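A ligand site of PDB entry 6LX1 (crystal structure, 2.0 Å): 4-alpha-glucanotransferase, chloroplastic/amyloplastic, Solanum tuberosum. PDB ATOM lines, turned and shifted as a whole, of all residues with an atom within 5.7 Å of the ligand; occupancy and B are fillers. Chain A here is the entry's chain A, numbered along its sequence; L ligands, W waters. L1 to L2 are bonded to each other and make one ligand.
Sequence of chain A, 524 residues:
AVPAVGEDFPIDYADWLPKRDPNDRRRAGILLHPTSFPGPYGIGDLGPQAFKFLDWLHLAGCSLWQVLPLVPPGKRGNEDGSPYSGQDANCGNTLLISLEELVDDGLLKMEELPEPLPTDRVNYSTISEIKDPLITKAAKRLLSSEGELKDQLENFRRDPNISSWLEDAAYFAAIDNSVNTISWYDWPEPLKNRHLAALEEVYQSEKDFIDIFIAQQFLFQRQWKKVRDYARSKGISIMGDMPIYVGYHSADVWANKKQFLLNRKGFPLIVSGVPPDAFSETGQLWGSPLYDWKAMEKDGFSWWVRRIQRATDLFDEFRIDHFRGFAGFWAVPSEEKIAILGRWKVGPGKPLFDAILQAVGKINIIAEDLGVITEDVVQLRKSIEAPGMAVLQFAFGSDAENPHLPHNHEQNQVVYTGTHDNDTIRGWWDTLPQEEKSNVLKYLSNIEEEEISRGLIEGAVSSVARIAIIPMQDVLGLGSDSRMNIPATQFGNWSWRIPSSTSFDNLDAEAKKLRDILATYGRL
OD2 of Asp 321 is covalently linked to C1 of LIG L1.
The side-chain amide nitrogen (NE2) of Gln 490 lies within hydrogen-bond range of an oxygen (O4) of LG2 L2 (2.7 Å).
The side-chain carboxylate (OD1) of Asp 421 is in hydrogen-bond range of an oxygen (O2) of LIG L1, 2.7 Å away.
A ring nitrogen (NE2) of His 420 lies within hydrogen-bond range of an oxygen (O1) of LIG L1, at 2.9 Å.
An oxygen (O1) of LG2 L2 lies within hydrogen-bond range of the side-chain amide nitrogen (ND2) of Asn 485.
An oxygen (O2) of LG2 L2 lies within hydrogen-bond range of the backbone NH (N) of Ala 488, 3.0 Å away.
The guanidinium group (NH2) of Arg 319 is in hydrogen-bond range of an oxygen (O1) of LIG L1.
The side-chain carboxylate of Asp 321 lies within salt-bridge range of the guanidinium group of Arg 319 (3.3 Å).
The backbone carbonyl oxygen (O) of Ala 488 sits at hydrogen-bond distance from the side-chain amide nitrogen (NE2) of Gln 490 (2.9 Å).
A ring nitrogen (NE2) of His 420 sits close to the side-chain carboxylate (OD1) of Asp 421, 3.4 Å away.
The side-chain amide nitrogen (ND2) of Asn 485 sits at hydrogen-bond distance from the side-chain carboxylate (OD1) of Asp 421 (2.9 Å).
O of His 420 is in hydrogen-bond range of N of Asn 485 (3.1 Å).
A ring nitrogen (NE2) of His 420 sits close to the side-chain hydroxyl (OH) of Tyr 84 (3.3 Å).
N of Tyr 84 lies close to OG of Ser 82 (3.1 Å).
The side-chain hydroxyl of Thr 489 lies within hydrogen-bond range of the backbone carbonyl oxygen of Ile 486.
Residues that only touch the ligand: Ser 85 (2.9 Å), Pro 487 (3.3 Å), Trp 494 (3.6 Å), Tyr 84 (3.7 Å), Ser 82 (3.7 Å) and Thr 489 (3.9 Å).
Hydrophobic or aromatic side chains within 4 Å of the ligand: Tyr 84, His 420, Pro 487 and Trp 494.
13 residues have an atom within 4 Å of the ligand: Ser 82, Tyr 84, Ser 85, Arg 319, Asp 321, His 420, Asp 421, Asn 485, Pro 487, Ala 488, Thr 489, Gln 490 and Trp 494.
The nearest printed residue that does not touch the ligand is Trp 286 (4.4 Å).
Water W1 lies within hydrogen-bond range of OG of Ser 82, O3 of LG2 L2 and NE1 of Trp 494.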
ATOM      1  N   SER A  82      -5.313 -27.098  13.888  1.00  0.00           N
ATOM      2  CA  SER A  82      -5.219 -26.195  15.067  1.00  0.00           C
ATOM      3  C   SER A  82      -5.729 -26.906  16.311  1.00  0.00           C
ATOM      4  O   SER A  82      -6.923 -27.204  16.397  1.00  0.00           O
ATOM      5  CB  SER A  82      -5.988 -24.922  14.909  1.00  0.00           C
ATOM      6  OG  SER A  82      -5.834 -24.165  16.093  1.00  0.00           O
ATOM      7  N   TYR A  84      -6.402 -25.376  18.918  1.00  0.00           N
ATOM      8  CA  TYR A  84      -7.229 -24.330  19.585  1.00  0.00           C
ATOM      9  C   TYR A  84      -8.579 -24.129  18.897  1.00  0.00           C
ATOM     10  O   TYR A  84      -9.350 -23.376  19.463  1.00  0.00           O
ATOM     11  CB  TYR A  84      -6.416 -23.029  19.742  1.00  0.00           C
ATOM     12  CG  TYR A  84      -5.220 -23.242  20.646  1.00  0.00           C
ATOM     13  CD1 TYR A  84      -5.307 -23.162  22.013  1.00  0.00           C
ATOM     14  CD2 TYR A  84      -3.989 -23.584  20.095  1.00  0.00           C
ATOM     15  CE1 TYR A  84      -4.200 -23.404  22.827  1.00  0.00           C
ATOM     16  CE2 TYR A  84      -2.881 -23.842  20.893  1.00  0.00           C
ATOM     17  CZ  TYR A  84      -3.000 -23.763  22.266  1.00  0.00           C
ATOM     18  OH  TYR A  84      -1.876 -24.012  23.017  1.00  0.00           O
ATOM     19  N   SER A  85      -8.884 -24.900  17.865  1.00  0.00           N
ATOM     20  CA  SER A  85     -10.150 -24.889  17.094  1.00  0.00           C
ATOM     21  C   SER A  85     -10.748 -26.290  17.157  1.00  0.00           C
ATOM     22  O   SER A  85     -11.006 -26.874  16.117  1.00  0.00           O
ATOM     23  CB  SER A  85      -9.872 -24.506  15.636  1.00  0.00           C
ATOM     24  OG  SER A  85      -9.340 -23.232  15.620  1.00  0.00           O
ATOM     25  N   ASP A 241      -3.178 -27.544  28.311  1.00  0.00           N
ATOM     26  CA  ASP A 241      -3.584 -26.195  27.884  1.00  0.00           C
ATOM     27  C   ASP A 241      -5.044 -26.278  27.465  1.00  0.00           C
ATOM     28  O   ASP A 241      -5.472 -27.311  26.960  1.00  0.00           O
ATOM     29  CB  ASP A 241      -2.722 -25.720  26.714  1.00  0.00           C
ATOM     30  CG  ASP A 241      -2.693 -24.228  26.464  1.00  0.00           C
ATOM     31  OD1 ASP A 241      -3.342 -23.446  27.237  1.00  0.00           O
ATOM     32  OD2 ASP A 241      -1.997 -23.842  25.478  1.00  0.00           O
ATOM     33  N   PRO A 243      -8.274 -23.587  25.733  1.00  0.00           N
ATOM     34  CA  PRO A 243      -8.785 -22.248  25.399  1.00  0.00           C
ATOM     35  C   PRO A 243      -9.881 -21.959  26.439  1.00  0.00           C
ATOM     36  O   PRO A 243     -10.619 -22.892  26.811  1.00  0.00           O
ATOM     37  CB  PRO A 243      -9.248 -22.391  23.933  1.00  0.00           C
ATOM     38  CG  PRO A 243      -9.531 -23.884  23.769  1.00  0.00           C
ATOM     39  CD  PRO A 243      -8.581 -24.614  24.705  1.00  0.00           C
ATOM     40  N   GLN A 284      -9.706  -7.845  16.851  1.00  0.00           N
ATOM     41  CA  GLN A 284      -9.710  -9.307  16.511  1.00  0.00           C
ATOM     42  C   GLN A 284     -11.095  -9.908  16.857  1.00  0.00           C
ATOM     43  O   GLN A 284     -11.510  -9.871  18.054  1.00  0.00           O
ATOM     44  CB  GLN A 284      -8.527  -9.963  17.219  1.00  0.00           C
ATOM     45  CG  GLN A 284      -7.932 -11.177  16.505  1.00  0.00           C
ATOM     46  CD  GLN A 284      -6.753 -11.757  17.258  1.00  0.00           C
ATOM     47  OE1 GLN A 284      -6.192 -11.136  18.156  1.00  0.00           O
ATOM     48  NE2 GLN A 284      -6.377 -12.983  16.928  1.00  0.00           N
ATOM     49  N   LEU A 285     -11.832 -10.386  15.844  1.00  0.00           N
ATOM     50  CA  LEU A 285     -13.122 -11.102  15.999  1.00  0.00           C
ATOM     51  C   LEU A 285     -12.836 -12.603  16.071  1.00  0.00           C
ATOM     52  O   LEU A 285     -12.583 -13.169  15.007  1.00  0.00           O
ATOM     53  CB  LEU A 285     -14.054 -10.790  14.824  1.00  0.00           C
ATOM     54  CG  LEU A 285     -15.410 -11.493  14.868  1.00  0.00           C
ATOM     55  CD1 LEU A 285     -16.230 -11.003  16.049  1.00  0.00           C
ATOM     56  CD2 LEU A 285     -16.185 -11.292  13.572  1.00  0.00           C
ATOM     57  N   TRP A 286     -12.892 -13.226  17.242  1.00  0.00           N
ATOM     58  CA  TRP A 286     -12.629 -14.683  17.402  1.00  0.00           C
ATOM     59  C   TRP A 286     -13.882 -15.491  17.091  1.00  0.00           C
ATOM     60  O   TRP A 286     -13.721 -16.530  16.502  1.00  0.00           O
ATOM     61  CB  TRP A 286     -12.126 -15.053  18.785  1.00  0.00           C
ATOM     62  CG  TRP A 286     -10.835 -14.415  19.155  1.00  0.00           C
ATOM     63  CD1 TRP A 286      -9.862 -13.934  18.316  1.00  0.00           C
ATOM     64  CD2 TRP A 286     -10.364 -14.222  20.495  1.00  0.00           C
ATOM     65  NE1 TRP A 286      -8.825 -13.425  19.059  1.00  0.00           N
ATOM     66  CE2 TRP A 286      -9.098 -13.594  20.395  1.00  0.00           C
ATOM     67  CE3 TRP A 286     -10.901 -14.498  21.754  1.00  0.00           C
ATOM     68  CZ2 TRP A 286      -8.369 -13.246  21.521  1.00  0.00           C
ATOM     69  CZ3 TRP A 286     -10.168 -14.158  22.870  1.00  0.00           C
ATOM     70  CH2 TRP A 286      -8.923 -13.527  22.741  1.00  0.00           C
ATOM     71  N   ARG A 319      -2.451 -24.730  31.596  1.00  0.00           N
ATOM     72  CA  ARG A 319      -2.659 -23.310  31.272  1.00  0.00           C
ATOM     73  C   ARG A 319      -4.123 -23.098  30.873  1.00  0.00           C
ATOM     74  O   ARG A 319      -4.707 -23.982  30.247  1.00  0.00           O
ATOM     75  CB  ARG A 319      -1.728 -22.913  30.134  1.00  0.00           C
ATOM     76  CG  ARG A 319      -1.642 -21.415  29.913  1.00  0.00           C
ATOM     77  CD  ARG A 319      -0.655 -21.128  28.787  1.00  0.00           C
ATOM     78  NE  ARG A 319      -1.314 -21.324  27.511  1.00  0.00           N
ATOM     79  CZ  ARG A 319      -1.070 -20.621  26.395  1.00  0.00           C
ATOM     80  NH1 ARG A 319      -0.114 -19.703  26.368  1.00  0.00           N
ATOM     81  NH2 ARG A 319      -1.755 -20.852  25.274  1.00  0.00           N
ATOM     82  N   ASP A 321      -5.785 -20.483  28.381  1.00  0.00           N
ATOM     83  CA  ASP A 321      -5.520 -19.409  27.388  1.00  0.00           C
ATOM     84  C   ASP A 321      -6.639 -18.363  27.485  1.00  0.00           C
ATOM     85  O   ASP A 321      -7.817 -18.731  27.510  1.00  0.00           O
ATOM     86  CB  ASP A 321      -5.367 -20.110  26.048  1.00  0.00           C
ATOM     87  CG  ASP A 321      -4.837 -19.304  24.881  1.00  0.00           C
ATOM     88  OD1 ASP A 321      -4.624 -18.106  25.042  1.00  0.00           O
ATOM     89  OD2 ASP A 321      -4.531 -19.951  23.826  1.00  0.00           O
ATOM     90  N   GLU A 368      -2.679 -17.671  31.516  1.00  0.00           N
ATOM     91  CA  GLU A 368      -2.108 -16.955  30.343  1.00  0.00           C
ATOM     92  C   GLU A 368      -2.555 -15.496  30.496  1.00  0.00           C
ATOM     93  O   GLU A 368      -3.767 -15.230  30.469  1.00  0.00           O
ATOM     94  CB  GLU A 368      -2.574 -17.547  29.006  1.00  0.00           C
ATOM     95  CG  GLU A 368      -2.052 -16.759  27.812  1.00  0.00           C
ATOM     96  CD  GLU A 368      -2.885 -15.532  27.391  1.00  0.00           C
ATOM     97  OE1 GLU A 368      -4.091 -15.699  27.057  1.00  0.00           O
ATOM     98  OE2 GLU A 368      -2.312 -14.407  27.300  1.00  0.00           O
ATOM     99  N   HIS A 420       4.618 -21.702  21.739  1.00  0.00           N
ATOM    100  CA  HIS A 420       4.259 -22.176  20.378  1.00  0.00           C
ATOM    101  C   HIS A 420       3.792 -21.003  19.488  1.00  0.00           C
ATOM    102  O   HIS A 420       3.784 -21.208  18.268  1.00  0.00           O
ATOM    103  CB  HIS A 420       3.166 -23.265  20.476  1.00  0.00           C
ATOM    104  CG  HIS A 420       1.957 -22.727  21.123  1.00  0.00           C
ATOM    105  ND1 HIS A 420       1.845 -22.618  22.504  1.00  0.00           N
ATOM    106  CD2 HIS A 420       0.846 -22.176  20.589  1.00  0.00           C
ATOM    107  CE1 HIS A 420       0.695 -22.068  22.766  1.00  0.00           C
ATOM    108  NE2 HIS A 420       0.097 -21.733  21.630  1.00  0.00           N
ATOM    109  N   ASP A 421       3.369 -19.873  20.066  1.00  0.00           N
ATOM    110  CA  ASP A 421       2.952 -18.643  19.333  1.00  0.00           C
ATOM    111  C   ASP A 421       4.155 -17.765  18.945  1.00  0.00           C
ATOM    112  O   ASP A 421       3.990 -16.817  18.126  1.00  0.00           O
ATOM    113  CB  ASP A 421       1.922 -17.843  20.137  1.00  0.00           C
ATOM    114  CG  ASP A 421       0.525 -18.467  20.207  1.00  0.00           C
ATOM    115  OD1 ASP A 421       0.188 -19.241  19.285  1.00  0.00           O
ATOM    116  OD2 ASP A 421      -0.157 -18.286  21.230  1.00  0.00           O
ATOM    117  N   ASN A 485       3.515 -21.989  15.291  1.00  0.00           N
ATOM    118  CA  ASN A 485       2.352 -21.144  14.934  1.00  0.00           C
ATOM    119  C   ASN A 485       2.821 -19.705  14.703  1.00  0.00           C
ATOM    120  O   ASN A 485       3.605 -19.188  15.521  1.00  0.00           O
ATOM    121  CB  ASN A 485       1.252 -21.160  15.996  1.00  0.00           C
ATOM    122  CG  ASN A 485       0.023 -20.385  15.617  1.00  0.00           C
ATOM    123  OD1 ASN A 485      -0.509 -20.590  14.523  1.00  0.00           O
ATOM    124  ND2 ASN A 485      -0.470 -19.533  16.487  1.00  0.00           N
ATOM    125  N   ILE A 486       2.309 -19.065  13.645  1.00  0.00           N
ATOM    126  CA  ILE A 486       2.322 -17.577  13.494  1.00  0.00           C
ATOM    127  C   ILE A 486       0.910 -17.090  13.768  1.00  0.00           C
ATOM    128  O   ILE A 486      -0.011 -17.339  12.991  1.00  0.00           O
ATOM    129  CB  ILE A 486       2.838 -17.139  12.095  1.00  0.00           C
ATOM    130  CG1 ILE A 486       4.190 -17.750  11.759  1.00  0.00           C
ATOM    131  CG2 ILE A 486       2.857 -15.613  12.039  1.00  0.00           C
ATOM    132  CD1 ILE A 486       4.693 -17.516  10.329  1.00  0.00           C
ATOM    133  N   PRO A 487       0.624 -16.440  14.904  1.00  0.00           N
ATOM    134  CA  PRO A 487      -0.739 -16.013  15.196  1.00  0.00           C
ATOM    135  C   PRO A 487      -1.474 -15.258  14.060  1.00  0.00           C
ATOM    136  O   PRO A 487      -0.881 -14.402  13.452  1.00  0.00           O
ATOM    137  CB  PRO A 487      -0.543 -15.109  16.399  1.00  0.00           C
ATOM    138  CG  PRO A 487       0.646 -15.735  17.116  1.00  0.00           C
ATOM    139  CD  PRO A 487       1.565 -16.162  16.003  1.00  0.00           C
ATOM    140  N   ALA A 488      -2.707 -15.674  13.800  1.00  0.00           N
ATOM    141  CA  ALA A 488      -3.645 -15.185  12.751  1.00  0.00           C
ATOM    142  C   ALA A 488      -3.297 -15.711  11.351  1.00  0.00           C
ATOM    143  O   ALA A 488      -4.151 -15.541  10.465  1.00  0.00           O
ATOM    144  CB  ALA A 488      -3.755 -13.684  12.790  1.00  0.00           C
ATOM    145  N   THR A 489      -2.163 -16.354  11.088  1.00  0.00           N
ATOM    146  CA  THR A 489      -1.886 -16.860   9.709  1.00  0.00           C
ATOM    147  C   THR A 489      -2.697 -18.136   9.451  1.00  0.00           C
ATOM    148  O   THR A 489      -3.205 -18.734  10.432  1.00  0.00           O
ATOM    149  CB  THR A 489      -0.394 -17.091   9.455  1.00  0.00           C
ATOM    150  OG1 THR A 489       0.074 -18.214  10.223  1.00  0.00           O
ATOM    151  CG2 THR A 489       0.384 -15.828   9.737  1.00  0.00           C
ATOM    152  N   GLN A 490      -2.850 -18.539   8.188  1.00  0.00           N
ATOM    153  CA  GLN A 490      -3.776 -19.646   7.847  1.00  0.00           C
ATOM    154  C   GLN A 490      -3.002 -20.896   7.422  1.00  0.00           C
ATOM    155  O   GLN A 490      -3.638 -21.913   7.369  1.00  0.00           O
ATOM    156  CB  GLN A 490      -4.782 -19.182   6.789  1.00  0.00           C
ATOM    157  CG  GLN A 490      -5.760 -18.152   7.312  1.00  0.00           C
ATOM    158  CD  GLN A 490      -6.244 -18.511   8.703  1.00  0.00           C
ATOM    159  OE1 GLN A 490      -7.148 -19.326   8.871  1.00  0.00           O
ATOM    160  NE2 GLN A 490      -5.615 -17.918   9.715  1.00  0.00           N
ATOM    161  N   TRP A 494       1.207 -25.604  13.019  1.00  0.00           N
ATOM    162  CA  TRP A 494       0.983 -26.856  13.799  1.00  0.00           C
ATOM    163  C   TRP A 494       1.590 -28.073  13.121  1.00  0.00           C
ATOM    164  O   TRP A 494       1.230 -29.166  13.529  1.00  0.00           O
ATOM    165  CB  TRP A 494      -0.532 -27.038  14.000  1.00  0.00           C
ATOM    166  CG  TRP A 494      -1.278 -25.788  14.344  1.00  0.00           C
ATOM    167  CD1 TRP A 494      -2.225 -25.172  13.606  1.00  0.00           C
ATOM    168  CD2 TRP A 494      -1.129 -24.994  15.535  1.00  0.00           C
ATOM    169  NE1 TRP A 494      -2.669 -24.046  14.225  1.00  0.00           N
ATOM    170  CE2 TRP A 494      -2.010 -23.909  15.414  1.00  0.00           C
ATOM    171  CE3 TRP A 494      -0.335 -25.096  16.681  1.00  0.00           C
ATOM    172  CZ2 TRP A 494      -2.130 -22.930  16.411  1.00  0.00           C
ATOM    173  CZ3 TRP A 494      -0.470 -24.148  17.675  1.00  0.00           C
ATOM    174  CH2 TRP A 494      -1.378 -23.085  17.551  1.00  0.00           C
HETATM  175  C1  LIG L   1      -4.278 -19.193  22.617  1.00  0.00           C
HETATM  176  C2  LIG L   1      -3.257 -19.965  21.816  1.00  0.00           C
HETATM  177  C3  LIG L   1      -3.203 -19.456  20.384  1.00  0.00           C
HETATM  178  C4  LIG L   1      -4.608 -19.515  19.765  1.00  0.00           C
HETATM  179  C5  LIG L   1      -5.521 -18.696  20.614  1.00  0.00           C
HETATM  180  C6  LIG L   1      -6.894 -18.585  19.965  1.00  0.00           C
HETATM  181  O1  LIG L   1      -1.967 -19.885  22.427  1.00  0.00           O
HETATM  182  O2  LIG L   1      -2.292 -20.224  19.617  1.00  0.00           O
HETATM  183  O3  LIG L   1      -4.571 -18.898  18.478  1.00  0.00           O
HETATM  184  O4  LIG L   1      -5.560 -19.251  21.946  1.00  0.00           O
HETATM  185  O5  LIG L   1      -7.857 -18.416  20.954  1.00  0.00           O
HETATM  186  C1  LG2 L   2      -4.321 -19.798  17.422  1.00  0.00           C
HETATM  187  O1  LG2 L   2      -2.976 -17.959  16.633  1.00  0.00           O
HETATM  188  C2  LG2 L   2      -3.972 -18.911  16.240  1.00  0.00           C
HETATM  189  C3  LG2 L   2     -10.401 -18.411  12.350  1.00  0.00           C
HETATM  190  C4  LG2 L   2      -5.219 -18.190  15.699  1.00  0.00           C
HETATM  191  O2  LG2 L   2      -4.774 -17.707  14.422  1.00  0.00           O
HETATM  192  C5  LG2 L   2      -6.346 -19.210  15.470  1.00  0.00           C
HETATM  193  N1  LG2 L   2      -7.482 -18.733  14.729  1.00  0.00           N
HETATM  194  C6  LG2 L   2      -6.700 -19.922  16.760  1.00  0.00           C
HETATM  195  O3  LG2 L   2      -5.472 -20.603  17.152  1.00  0.00           O
HETATM  196  C7  LG2 L   2      -7.778 -21.013  16.568  1.00  0.00           C
HETATM  197  C8  LG2 L   2      -7.917 -19.515  13.529  1.00  0.00           C
HETATM  198  C9  LG2 L   2      -7.933 -18.601  12.314  1.00  0.00           C
HETATM  199  O4  LG2 L   2      -6.620 -18.024  12.180  1.00  0.00           O
HETATM  200  C10 LG2 L   2      -9.114 -17.630  12.536  1.00  0.00           C
HETATM  201  O5  LG2 L   2      -9.152 -16.522  11.614  1.00  0.00           O
HETATM  202  O6  LG2 L   2     -11.422 -17.575  12.889  1.00  0.00           O
HETATM  203  C11 LG2 L   2     -10.365 -19.792  13.000  1.00  0.00           C
HETATM  204  C12 LG2 L   2      -9.229 -20.273  13.567  1.00  0.00           C
HETATM  205  C13 LG2 L   2     -11.592 -20.692  12.938  1.00  0.00           C
HETATM  206  O7  LG2 L   2     -12.352 -20.630  14.148  1.00  0.00           O
HETATM  207  O   HOH W   1      -5.107 -21.903  14.327  1.00  0.00           O
HETATM  208  O   HOH W   2      -8.378 -16.791  16.849  1.00  0.00           O
HETATM  209  O   HOH W   3      -8.208 -18.872  23.994  1.00  0.00           O
HETATM  210  O   HOH W   4     -10.143 -18.179  19.632  1.00  0.00           O
HETATM  211  O   HOH W   5      -3.604 -15.950  18.247  1.00  0.00           O
HETATM  212  O   HOH W   6      -2.599 -19.653  13.194  1.00  0.00           O
